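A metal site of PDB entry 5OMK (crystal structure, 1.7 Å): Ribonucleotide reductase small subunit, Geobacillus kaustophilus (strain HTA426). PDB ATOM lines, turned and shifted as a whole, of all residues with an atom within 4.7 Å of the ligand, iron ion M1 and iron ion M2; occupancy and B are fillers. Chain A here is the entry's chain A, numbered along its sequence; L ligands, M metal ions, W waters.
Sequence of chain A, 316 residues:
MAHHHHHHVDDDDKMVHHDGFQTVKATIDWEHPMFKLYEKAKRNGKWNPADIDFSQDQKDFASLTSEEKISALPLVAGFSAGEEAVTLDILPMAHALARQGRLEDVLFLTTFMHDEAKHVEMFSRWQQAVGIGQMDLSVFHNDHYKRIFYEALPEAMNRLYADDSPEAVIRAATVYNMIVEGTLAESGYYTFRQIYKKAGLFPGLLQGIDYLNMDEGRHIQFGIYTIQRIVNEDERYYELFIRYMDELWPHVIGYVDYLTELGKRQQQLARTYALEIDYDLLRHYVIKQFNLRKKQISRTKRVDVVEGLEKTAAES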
ATOM      1  N   LEU A  75      21.022 -13.269 -26.882  1.00  0.00           N
ATOM      2  CA  LEU A  75      21.742 -12.717 -25.737  1.00  0.00           C
ATOM      3  C   LEU A  75      21.720 -11.190 -25.767  1.00  0.00           C
ATOM      4  O   LEU A  75      21.502 -10.559 -24.728  1.00  0.00           O
ATOM      5  CB  LEU A  75      23.171 -13.242 -25.704  1.00  0.00           C
ATOM      6  CG  LEU A  75      23.985 -12.952 -24.440  1.00  0.00           C
ATOM      7  CD1 LEU A  75      23.272 -13.542 -23.220  1.00  0.00           C
ATOM      8  CD2 LEU A  75      25.438 -13.522 -24.574  1.00  0.00           C
ATOM      9  N   GLY A  78      18.331  -9.999 -24.822  1.00  0.00           N
ATOM     10  CA  GLY A  78      18.152  -9.993 -23.380  1.00  0.00           C
ATOM     11  C   GLY A  78      18.833  -8.807 -22.732  1.00  0.00           C
ATOM     12  O   GLY A  78      18.274  -8.169 -21.835  1.00  0.00           O
ATOM     13  N   PHE A  79      20.053  -8.475 -23.175  1.00  0.00           N
ATOM     14  CA  PHE A  79      20.768  -7.376 -22.545  1.00  0.00           C
ATOM     15  C   PHE A  79      20.134  -6.026 -22.854  1.00  0.00           C
ATOM     16  O   PHE A  79      19.943  -5.219 -21.943  1.00  0.00           O
ATOM     17  CB  PHE A  79      22.240  -7.391 -22.922  1.00  0.00           C
ATOM     18  CG  PHE A  79      23.108  -8.079 -21.895  1.00  0.00           C
ATOM     19  CD1 PHE A  79      23.433  -7.442 -20.708  1.00  0.00           C
ATOM     20  CD2 PHE A  79      23.597  -9.348 -22.108  1.00  0.00           C
ATOM     21  CE1 PHE A  79      24.219  -8.065 -19.754  1.00  0.00           C
ATOM     22  CE2 PHE A  79      24.400  -9.973 -21.168  1.00  0.00           C
ATOM     23  CZ  PHE A  79      24.713  -9.341 -19.988  1.00  0.00           C
ATOM     24  N   GLY A  82      17.177  -5.511 -20.955  1.00  0.00           N
ATOM     25  CA  GLY A  82      17.548  -5.449 -19.557  1.00  0.00           C
ATOM     26  C   GLY A  82      18.080  -4.082 -19.158  1.00  0.00           C
ATOM     27  O   GLY A  82      17.690  -3.542 -18.121  1.00  0.00           O
ATOM     28  N   GLU A  83      19.003  -3.536 -19.969  1.00  0.00           N
ATOM     29  CA  GLU A  83      19.594  -2.225 -19.698  1.00  0.00           C
ATOM     30  C   GLU A  83      18.530  -1.140 -19.715  1.00  0.00           C
ATOM     31  O   GLU A  83      18.523  -0.240 -18.862  1.00  0.00           O
ATOM     32  CB  GLU A  83      20.669  -1.862 -20.709  1.00  0.00           C
ATOM     33  CG  GLU A  83      21.775  -2.864 -20.931  1.00  0.00           C
ATOM     34  CD  GLU A  83      22.632  -3.175 -19.702  1.00  0.00           C
ATOM     35  OE1 GLU A  83      23.356  -4.199 -19.738  1.00  0.00           O
ATOM     36  OE2 GLU A  83      22.590  -2.413 -18.701  1.00  0.00           O
ATOM     37  N   VAL A  86      16.236  -1.450 -16.515  1.00  0.00           N
ATOM     38  CA  VAL A  86      16.871  -0.939 -15.284  1.00  0.00           C
ATOM     39  C   VAL A  86      17.137   0.572 -15.343  1.00  0.00           C
ATOM     40  O   VAL A  86      17.112   1.252 -14.312  1.00  0.00           O
ATOM     41  CB  VAL A  86      18.168  -1.716 -14.947  1.00  0.00           C
ATOM     42  CG1 VAL A  86      17.849  -3.162 -14.709  1.00  0.00           C
ATOM     43  CG2 VAL A  86      19.218  -1.559 -16.031  1.00  0.00           C
ATOM     44  N   PHE A 112      24.783   5.368 -10.819  1.00  0.00           N
ATOM     45  CA  PHE A 112      24.088   4.138 -11.197  1.00  0.00           C
ATOM     46  C   PHE A 112      23.203   4.363 -12.437  1.00  0.00           C
ATOM     47  O   PHE A 112      23.304   3.645 -13.439  1.00  0.00           O
ATOM     48  CB  PHE A 112      23.268   3.689  -9.974  1.00  0.00           C
ATOM     49  CG  PHE A 112      22.786   2.252  -9.974  1.00  0.00           C
ATOM     50  CD1 PHE A 112      22.750   1.543  -8.783  1.00  0.00           C
ATOM     51  CD2 PHE A 112      22.298   1.645 -11.105  1.00  0.00           C
ATOM     52  CE1 PHE A 112      22.296   0.241  -8.726  1.00  0.00           C
ATOM     53  CE2 PHE A 112      21.822   0.337 -11.050  1.00  0.00           C
ATOM     54  CZ  PHE A 112      21.812  -0.359  -9.872  1.00  0.00           C
ATOM     55  N   GLU A 116      23.674   2.929 -16.385  1.00  0.00           N
ATOM     56  CA  GLU A 116      22.700   2.140 -17.143  1.00  0.00           C
ATOM     57  C   GLU A 116      22.355   2.801 -18.453  1.00  0.00           C
ATOM     58  O   GLU A 116      22.187   2.099 -19.464  1.00  0.00           O
ATOM     59  CB  GLU A 116      21.444   1.895 -16.299  1.00  0.00           C
ATOM     60  CG  GLU A 116      21.681   1.146 -14.989  1.00  0.00           C
ATOM     61  CD  GLU A 116      22.234  -0.286 -15.150  1.00  0.00           C
ATOM     62  OE1 GLU A 116      22.256  -1.005 -14.139  1.00  0.00           O
ATOM     63  OE2 GLU A 116      22.588  -0.721 -16.267  1.00  0.00           O
ATOM     64  N   HIS A 119      24.925   1.874 -20.718  1.00  0.00           N
ATOM     65  CA  HIS A 119      24.789   0.484 -21.140  1.00  0.00           C
ATOM     66  C   HIS A 119      23.757   0.346 -22.250  1.00  0.00           C
ATOM     67  O   HIS A 119      23.977  -0.400 -23.218  1.00  0.00           O
ATOM     68  CB  HIS A 119      24.367  -0.429 -19.988  1.00  0.00           C
ATOM     69  CG  HIS A 119      25.319  -0.435 -18.839  1.00  0.00           C
ATOM     70  ND1 HIS A 119      25.066  -1.129 -17.660  1.00  0.00           N
ATOM     71  CD2 HIS A 119      26.499   0.191 -18.666  1.00  0.00           C
ATOM     72  CE1 HIS A 119      26.082  -0.951 -16.844  1.00  0.00           C
ATOM     73  NE2 HIS A 119      26.945  -0.117 -17.401  1.00  0.00           N
ATOM     74  N   TYR A 145      11.362 -14.587 -19.339  1.00  0.00           N
ATOM     75  CA  TYR A 145      12.048 -13.315 -19.404  1.00  0.00           C
ATOM     76  C   TYR A 145      11.072 -12.160 -19.162  1.00  0.00           C
ATOM     77  O   TYR A 145      11.364 -11.225 -18.386  1.00  0.00           O
ATOM     78  CB  TYR A 145      12.736 -13.173 -20.762  1.00  0.00           C
ATOM     79  CG  TYR A 145      13.529 -11.889 -20.885  1.00  0.00           C
ATOM     80  CD1 TYR A 145      14.903 -11.857 -20.637  1.00  0.00           C
ATOM     81  CD2 TYR A 145      12.883 -10.715 -21.250  1.00  0.00           C
ATOM     82  CE1 TYR A 145      15.606 -10.684 -20.743  1.00  0.00           C
ATOM     83  CE2 TYR A 145      13.571  -9.537 -21.366  1.00  0.00           C
ATOM     84  CZ  TYR A 145      14.938  -9.513 -21.078  1.00  0.00           C
ATOM     85  OH  TYR A 145      15.617  -8.350 -21.196  1.00  0.00           O
ATOM     86  N   PHE A 149      11.408  -9.073 -16.465  1.00  0.00           N
ATOM     87  CA  PHE A 149      11.753  -7.733 -16.947  1.00  0.00           C
ATOM     88  C   PHE A 149      10.556  -6.881 -17.343  1.00  0.00           C
ATOM     89  O   PHE A 149      10.598  -5.654 -17.162  1.00  0.00           O
ATOM     90  CB  PHE A 149      12.700  -7.865 -18.136  1.00  0.00           C
ATOM     91  CG  PHE A 149      14.074  -8.294 -17.724  1.00  0.00           C
ATOM     92  CD1 PHE A 149      14.995  -7.339 -17.281  1.00  0.00           C
ATOM     93  CD2 PHE A 149      14.469  -9.648 -17.762  1.00  0.00           C
ATOM     94  CE1 PHE A 149      16.249  -7.717 -16.868  1.00  0.00           C
ATOM     95  CE2 PHE A 149      15.750 -10.013 -17.361  1.00  0.00           C
ATOM     96  CZ  PHE A 149      16.649  -9.029 -16.913  1.00  0.00           C
ATOM     97  N   VAL A 180      18.355  -9.556 -11.246  1.00  0.00           N
ATOM     98  CA  VAL A 180      18.602  -9.045 -12.592  1.00  0.00           C
ATOM     99  C   VAL A 180      20.104  -8.773 -12.797  1.00  0.00           C
ATOM    100  O   VAL A 180      20.690  -9.186 -13.809  1.00  0.00           O
ATOM    101  CB  VAL A 180      17.736  -7.783 -12.831  1.00  0.00           C
ATOM    102  CG1 VAL A 180      18.276  -6.898 -13.948  1.00  0.00           C
ATOM    103  CG2 VAL A 180      16.284  -8.209 -13.102  1.00  0.00           C
ATOM    104  N   GLU A 181      20.723  -8.043 -11.880  1.00  0.00           N
ATOM    105  CA  GLU A 181      22.152  -7.712 -12.000  1.00  0.00           C
ATOM    106  C   GLU A 181      23.034  -8.846 -11.482  1.00  0.00           C
ATOM    107  O   GLU A 181      23.907  -9.370 -12.191  1.00  0.00           O
ATOM    108  CB  GLU A 181      22.451  -6.421 -11.233  1.00  0.00           C
ATOM    109  CG  GLU A 181      21.765  -5.237 -11.815  1.00  0.00           C
ATOM    110  CD  GLU A 181      22.062  -3.951 -11.090  1.00  0.00           C
ATOM    111  OE1 GLU A 181      22.030  -3.944  -9.847  1.00  0.00           O
ATOM    112  OE2 GLU A 181      22.377  -2.959 -11.762  1.00  0.00           O
ATOM    113  N   LEU A 184      21.596 -12.614 -13.339  1.00  0.00           N
ATOM    114  CA  LEU A 184      21.458 -12.682 -14.799  1.00  0.00           C
ATOM    115  C   LEU A 184      22.535 -11.875 -15.518  1.00  0.00           C
ATOM    116  O   LEU A 184      23.247 -12.421 -16.374  1.00  0.00           O
ATOM    117  CB  LEU A 184      20.063 -12.246 -15.209  1.00  0.00           C
ATOM    118  CG  LEU A 184      18.917 -13.202 -14.879  1.00  0.00           C
ATOM    119  CD1 LEU A 184      17.556 -12.546 -15.123  1.00  0.00           C
ATOM    120  CD2 LEU A 184      19.020 -14.486 -15.707  1.00  0.00           C
ATOM    121  N   ALA A 185      22.713 -10.598 -15.194  1.00  0.00           N
ATOM    122  CA  ALA A 185      23.737  -9.801 -15.882  1.00  0.00           C
ATOM    123  C   ALA A 185      25.124 -10.427 -15.748  1.00  0.00           C
ATOM    124  O   ALA A 185      25.893 -10.518 -16.726  1.00  0.00           O
ATOM    125  CB  ALA A 185      23.770  -8.356 -15.342  1.00  0.00           C
ATOM    126  N   SER A 187      25.996 -13.515 -15.189  1.00  0.00           N
ATOM    127  CA  SER A 187      26.102 -14.733 -15.990  1.00  0.00           C
ATOM    128  C   SER A 187      26.163 -14.374 -17.465  1.00  0.00           C
ATOM    129  O   SER A 187      26.868 -15.010 -18.236  1.00  0.00           O
ATOM    130  CB  SER A 187      24.919 -15.656 -15.698  1.00  0.00           C
ATOM    131  OG  SER A 187      24.865 -15.961 -14.315  1.00  0.00           O
ATOM    132  N   GLY A 188      25.452 -13.326 -17.870  1.00  0.00           N
ATOM    133  CA  GLY A 188      25.556 -12.892 -19.255  1.00  0.00           C
ATOM    134  C   GLY A 188      26.953 -12.447 -19.640  1.00  0.00           C
ATOM    135  O   GLY A 188      27.394 -12.693 -20.761  1.00  0.00           O
ATOM    136  N   TYR A 189      27.622 -11.711 -18.762  1.00  0.00           N
ATOM    137  CA  TYR A 189      28.988 -11.282 -19.052  1.00  0.00           C
ATOM    138  C   TYR A 189      29.871 -12.489 -19.235  1.00  0.00           C
ATOM    139  O   TYR A 189      30.671 -12.572 -20.179  1.00  0.00           O
ATOM    140  CB  TYR A 189      29.551 -10.428 -17.914  1.00  0.00           C
ATOM    141  CG  TYR A 189      28.742  -9.186 -17.621  1.00  0.00           C
ATOM    142  CD1 TYR A 189      28.158  -8.481 -18.646  1.00  0.00           C
ATOM    143  CD2 TYR A 189      28.579  -8.732 -16.297  1.00  0.00           C
ATOM    144  CE1 TYR A 189      27.435  -7.350 -18.408  1.00  0.00           C
ATOM    145  CE2 TYR A 189      27.844  -7.617 -16.038  1.00  0.00           C
ATOM    146  CZ  TYR A 189      27.260  -6.913 -17.096  1.00  0.00           C
ATOM    147  OH  TYR A 189      26.522  -5.768 -16.871  1.00  0.00           O
ATOM    148  N   THR A 191      28.937 -15.504 -20.072  1.00  0.00           N
ATOM    149  CA  THR A 191      28.550 -16.203 -21.304  1.00  0.00           C
ATOM    150  C   THR A 191      29.172 -15.546 -22.527  1.00  0.00           C
ATOM    151  O   THR A 191      29.750 -16.241 -23.383  1.00  0.00           O
ATOM    152  CB  THR A 191      27.025 -16.268 -21.407  1.00  0.00           C
ATOM    153  OG1 THR A 191      26.495 -16.934 -20.262  1.00  0.00           O
ATOM    154  CG2 THR A 191      26.560 -16.990 -22.629  1.00  0.00           C
ATOM    155  N   GLU A 216      29.010  -2.951 -13.039  1.00  0.00           N
ATOM    156  CA  GLU A 216      28.045  -3.787 -12.340  1.00  0.00           C
ATOM    157  C   GLU A 216      28.453  -4.058 -10.923  1.00  0.00           C
ATOM    158  O   GLU A 216      27.597  -4.223 -10.058  1.00  0.00           O
ATOM    159  CB  GLU A 216      27.862  -5.134 -13.060  1.00  0.00           C
ATOM    160  CG  GLU A 216      26.539  -5.771 -12.827  1.00  0.00           C
ATOM    161  CD  GLU A 216      25.448  -4.990 -13.505  1.00  0.00           C
ATOM    162  OE1 GLU A 216      25.329  -5.108 -14.758  1.00  0.00           O
ATOM    163  OE2 GLU A 216      24.791  -4.183 -12.799  1.00  0.00           O
ATOM    164  N   HIS A 219      26.866  -1.516  -8.785  1.00  0.00           N
ATOM    165  CA  HIS A 219      25.419  -1.718  -8.716  1.00  0.00           C
ATOM    166  C   HIS A 219      25.070  -2.814  -7.720  1.00  0.00           C
ATOM    167  O   HIS A 219      24.167  -2.673  -6.883  1.00  0.00           O
ATOM    168  CB  HIS A 219      24.881  -2.081 -10.128  1.00  0.00           C
ATOM    169  CG  HIS A 219      25.206  -1.055 -11.154  1.00  0.00           C
ATOM    170  ND1 HIS A 219      24.820  -1.169 -12.480  1.00  0.00           N
ATOM    171  CD2 HIS A 219      25.933   0.087 -11.063  1.00  0.00           C
ATOM    172  CE1 HIS A 219      25.289  -0.123 -13.151  1.00  0.00           C
ATOM    173  NE2 HIS A 219      25.954   0.652 -12.312  1.00  0.00           N
ATOM    174  N   TYR A 255      14.410 -18.855 -18.183  1.00  0.00           N
ATOM    175  CA  TYR A 255      14.992 -18.091 -19.271  1.00  0.00           C
ATOM    176  C   TYR A 255      16.324 -18.709 -19.699  1.00  0.00           C
ATOM    177  O   TYR A 255      16.620 -18.807 -20.899  1.00  0.00           O
ATOM    178  CB  TYR A 255      15.171 -16.642 -18.830  1.00  0.00           C
ATOM    179  CG  TYR A 255      15.874 -15.770 -19.841  1.00  0.00           C
ATOM    180  CD1 TYR A 255      15.373 -15.621 -21.124  1.00  0.00           C
ATOM    181  CD2 TYR A 255      17.028 -15.076 -19.499  1.00  0.00           C
ATOM    182  CE1 TYR A 255      16.028 -14.799 -22.066  1.00  0.00           C
ATOM    183  CE2 TYR A 255      17.684 -14.241 -20.437  1.00  0.00           C
ATOM    184  CZ  TYR A 255      17.170 -14.108 -21.697  1.00  0.00           C
ATOM    185  OH  TYR A 255      17.794 -13.306 -22.645  1.00  0.00           O
ATOM    186  N   VAL A 256      17.144 -19.105 -18.738  1.00  0.00           N
ATOM    187  CA  VAL A 256      18.435 -19.726 -19.063  1.00  0.00           C
ATOM    188  C   VAL A 256      18.214 -20.974 -19.904  1.00  0.00           C
ATOM    189  O   VAL A 256      18.878 -21.185 -20.913  1.00  0.00           O
ATOM    190  CB  VAL A 256      19.224 -20.020 -17.778  1.00  0.00           C
ATOM    191  CG1 VAL A 256      20.442 -20.895 -18.074  1.00  0.00           C
ATOM    192  CG2 VAL A 256      19.707 -18.734 -17.128  1.00  0.00           C
ATOM    193  N   LEU A 259      17.387 -20.022 -23.507  1.00  0.00           N
ATOM    194  CA  LEU A 259      18.540 -19.616 -24.300  1.00  0.00           C
ATOM    195  C   LEU A 259      19.427 -20.814 -24.634  1.00  0.00           C
ATOM    196  O   LEU A 259      20.009 -20.865 -25.722  1.00  0.00           O
ATOM    197  CB  LEU A 259      19.371 -18.592 -23.558  1.00  0.00           C
ATOM    198  CG  LEU A 259      18.728 -17.234 -23.340  1.00  0.00           C
ATOM    199  CD1 LEU A 259      19.729 -16.431 -22.529  1.00  0.00           C
ATOM    200  CD2 LEU A 259      18.409 -16.562 -24.662  1.00  0.00           C
ATOM    201  N   THR A 260      19.586 -21.731 -23.679  1.00  0.00           N
ATOM    202  CA  THR A 260      20.362 -22.934 -23.934  1.00  0.00           C
ATOM    203  C   THR A 260      19.728 -23.762 -25.052  1.00  0.00           C
ATOM    204  O   THR A 260      20.426 -24.224 -25.963  1.00  0.00           O
ATOM    205  CB  THR A 260      20.447 -23.760 -22.660  1.00  0.00           C
ATOM    206  OG1 THR A 260      21.228 -23.047 -21.703  1.00  0.00           O
ATOM    207  CG2 THR A 260      21.109 -25.132 -22.956  1.00  0.00           C
ATOM    208  N   TYR A 279      27.194 -25.663 -22.352  1.00  0.00           N
ATOM    209  CA  TYR A 279      25.973 -25.117 -21.767  1.00  0.00           C
ATOM    210  C   TYR A 279      25.749 -25.629 -20.349  1.00  0.00           C
ATOM    211  O   TYR A 279      25.262 -24.894 -19.492  1.00  0.00           O
ATOM    212  CB  TYR A 279      24.766 -25.426 -22.653  1.00  0.00           C
ATOM    213  CG  TYR A 279      24.813 -24.646 -23.923  1.00  0.00           C
ATOM    214  CD1 TYR A 279      24.628 -23.281 -23.916  1.00  0.00           C
ATOM    215  CD2 TYR A 279      25.079 -25.267 -25.137  1.00  0.00           C
ATOM    216  CE1 TYR A 279      24.694 -22.543 -25.072  1.00  0.00           C
ATOM    217  CE2 TYR A 279      25.140 -24.536 -26.311  1.00  0.00           C
ATOM    218  CZ  TYR A 279      24.946 -23.170 -26.268  1.00  0.00           C
ATOM    219  OH  TYR A 279      25.015 -22.428 -27.416  1.00  0.00           O
ATOM    220  N   LEU A 282      27.669 -23.206 -18.289  1.00  0.00           N
ATOM    221  CA  LEU A 282      26.990 -21.926 -18.173  1.00  0.00           C
ATOM    222  C   LEU A 282      25.827 -22.038 -17.199  1.00  0.00           C
ATOM    223  O   LEU A 282      25.632 -21.168 -16.348  1.00  0.00           O
ATOM    224  CB  LEU A 282      26.506 -21.457 -19.541  1.00  0.00           C
ATOM    225  CG  LEU A 282      27.574 -21.154 -20.592  1.00  0.00           C
ATOM    226  CD1 LEU A 282      26.933 -20.814 -21.928  1.00  0.00           C
ATOM    227  CD2 LEU A 282      28.528 -20.046 -20.134  1.00  0.00           C
ATOM    228  N   VAL A 286      25.227 -19.867 -13.507  1.00  0.00           N
ATOM    229  CA  VAL A 286      24.018 -19.167 -13.071  1.00  0.00           C
ATOM    230  C   VAL A 286      23.622 -19.615 -11.676  1.00  0.00           C
ATOM    231  O   VAL A 286      23.343 -18.787 -10.805  1.00  0.00           O
ATOM    232  CB  VAL A 286      22.862 -19.399 -14.072  1.00  0.00           C
ATOM    233  CG1 VAL A 286      21.568 -18.774 -13.557  1.00  0.00           C
ATOM    234  CG2 VAL A 286      23.202 -18.820 -15.406  1.00  0.00           C
HETATM  235  C1  LIG L   1      21.868  -4.165 -15.710  1.00  0.00           C
HETATM  236  O1  LIG L   1      22.225  -3.612 -16.769  1.00  0.00           O
HETATM  237  O2  LIG L   1      22.098  -3.789 -14.498  1.00  0.00           O
HETATM  238  C2  LIG L   1      21.011  -5.465 -15.889  1.00  0.00           C
HETATM  239  C3  LIG L   1      21.022  -6.080 -17.236  1.00  0.00           C
HETATM  240  C4  LIG L   1      20.242  -7.390 -17.342  1.00  0.00           C
HETATM  241  C5  LIG L   1      20.617  -8.257 -18.549  1.00  0.00           C
HETATM  242  C6  LIG L   1      19.709  -9.436 -18.753  1.00  0.00           C
HETATM  243  C7  LIG L   1      20.081 -10.377 -19.894  1.00  0.00           C
HETATM  244  C8  LIG L   1      21.276 -11.149 -19.576  1.00  0.00           C
HETATM  245  C9  LIG L   1      21.403 -12.433 -20.332  1.00  0.00           C
HETATM  246  C10 LIG L   1      21.407 -13.635 -19.380  1.00  0.00           C
HETATM  247  C11 LIG L   1      22.259 -14.730 -19.860  1.00  0.00           C
HETATM  248  C12 LIG L   1      22.419 -15.849 -18.830  1.00  0.00           C
HETATM  249  C13 LIG L   1      23.343 -16.954 -19.349  1.00  0.00           C
HETATM  250  C14 LIG L   1      22.633 -18.156 -19.993  1.00  0.00           C
HETATM  251  C15 LIG L   1      23.565 -19.106 -20.772  1.00  0.00           C
HETATM  252  C16 LIG L   1      23.074 -19.465 -22.199  1.00  0.00           C
HETATM  253 FE    FE M   1      23.431  -2.631 -13.472  1.00  0.00          FE
HETATM  254 FE    FE M   2      23.608  -2.387 -16.944  1.00  0.00          FE
HETATM  255  O   HOH W   1      24.774  -4.084 -17.761  1.00  0.00           O
HETATM  256  O   HOH W   2      24.577  -2.654 -15.159  1.00  0.00           O
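The backbone NH of Gly 82 is in hydrogen-bond range of the side-chain hydroxyl of Tyr 145, 3.2 Å away. The backbone carbonyl oxygen of Ser 187 lies within hydrogen-bond range of the side-chain hydroxyl of Thr 191 (2.8 Å). OE1 of Glu 216 lies within hydrogen-bond range of OH of Tyr 189, 2.5 Å away. The backbone carbonyl oxygen of Val 180 is in hydrogen-bond range of the backbone NH of Ala 185, 2.8 Å away. The backbone carbonyl oxygen of Gly 78 sits at hydrogen-bond distance from the side-chain hydroxyl of Tyr 145 (2.7 Å). The backbone carbonyl oxygen (O) of Val 256 is in hydrogen-bond range of the side-chain hydroxyl (OG1) of Thr 260 (3.1 Å).
Leu 75 touches the ligand. Gly 78 touches the ligand (O to C7, 3.5 Å). CD1 of Phe 79 touches C5 of the ligand, at 3.6 Å. CA of Gly 82 touches C4 of the ligand (3.99 Å). Val 86 touches the ligand. CZ of Phe 149 touches C6 of the ligand, at 3.6 Å. CG1 of Val 180 touches C2 of the ligand, at 3.6 Å. Leu 184 touches the ligand. Gly 188 touches the ligand (CA to C11, 3.8 Å). Thr 191 touches the ligand (OG1 to C13, 3.3 Å). Tyr 255 touches the ligand (CE2 to C10, 3.9 Å). Val 256 touches the ligand. Leu 282 touches the ligand (CD1 to C15, 3.9 Å). Hydrophobic or aromatic side chains within 4 Å of the ligand: Leu 75, Phe 79, Val 86, Phe 149, Val 180, Tyr 255, Val 256 and Leu 282. Within 4 Å of the ligand: Leu 75, Gly 78, Phe 79, Gly 82, Glu 83, Val 86, Glu 116, His 119, Phe 149, Val 180, Glu 181, Leu 184, Gly 188, Thr 191, Glu 216, Tyr 255, Val 256 and Leu 282. The nearest printed residue that does not touch the ligand is Ser 187 (4.01 Å).
Of the 28 residues printed, 4 come within 4 Å of iron ion M1. The nearest printed residue that does not touch iron ion M1 is Phe 112 (4.2 Å).
Four residues have an atom within 4 Å of iron ion M2: Glu 83, Glu 116, His 119 and Glu 216. The nearest printed residue that does not touch iron ion M2 is Tyr 189 (4.5 Å).
Iron ion M1 is bound by OE2 of Glu 181, at 2.0 Å. Iron ion M1 is bound by water W2 (2.0 Å). An oxygen (O2) of the ligand is bound to iron ion M1 (2.0 Å). The side-chain carboxylate (OE1) of Glu 116 binds iron ion M1 (2.1 Å). The side-chain carboxylate (OE2) of Glu 216 binds iron ion M1 (2.2 Å). ND1 of His 219 is bound to iron ion M1 (2.2 Å). Iron ion M1 has six donor atoms within binding distance.
Iron ion M2 is bound by an oxygen (O1) of the ligand (1.9 Å), the side-chain carboxylate of Glu 83 (2.0 Å), water W2 (2.0 Å), a ring nitrogen (ND1) of His 119 (2.1 Å), the side-chain carboxylate of Glu 116 (2.1 Å) and water W1 (2.2 Å).
Water W1 lies within hydrogen-bond range of OE1 of Glu 83 (2.4 Å), OH of Tyr 189 (2.6 Å) and OE1 of Glu 216 (3.2 Å).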
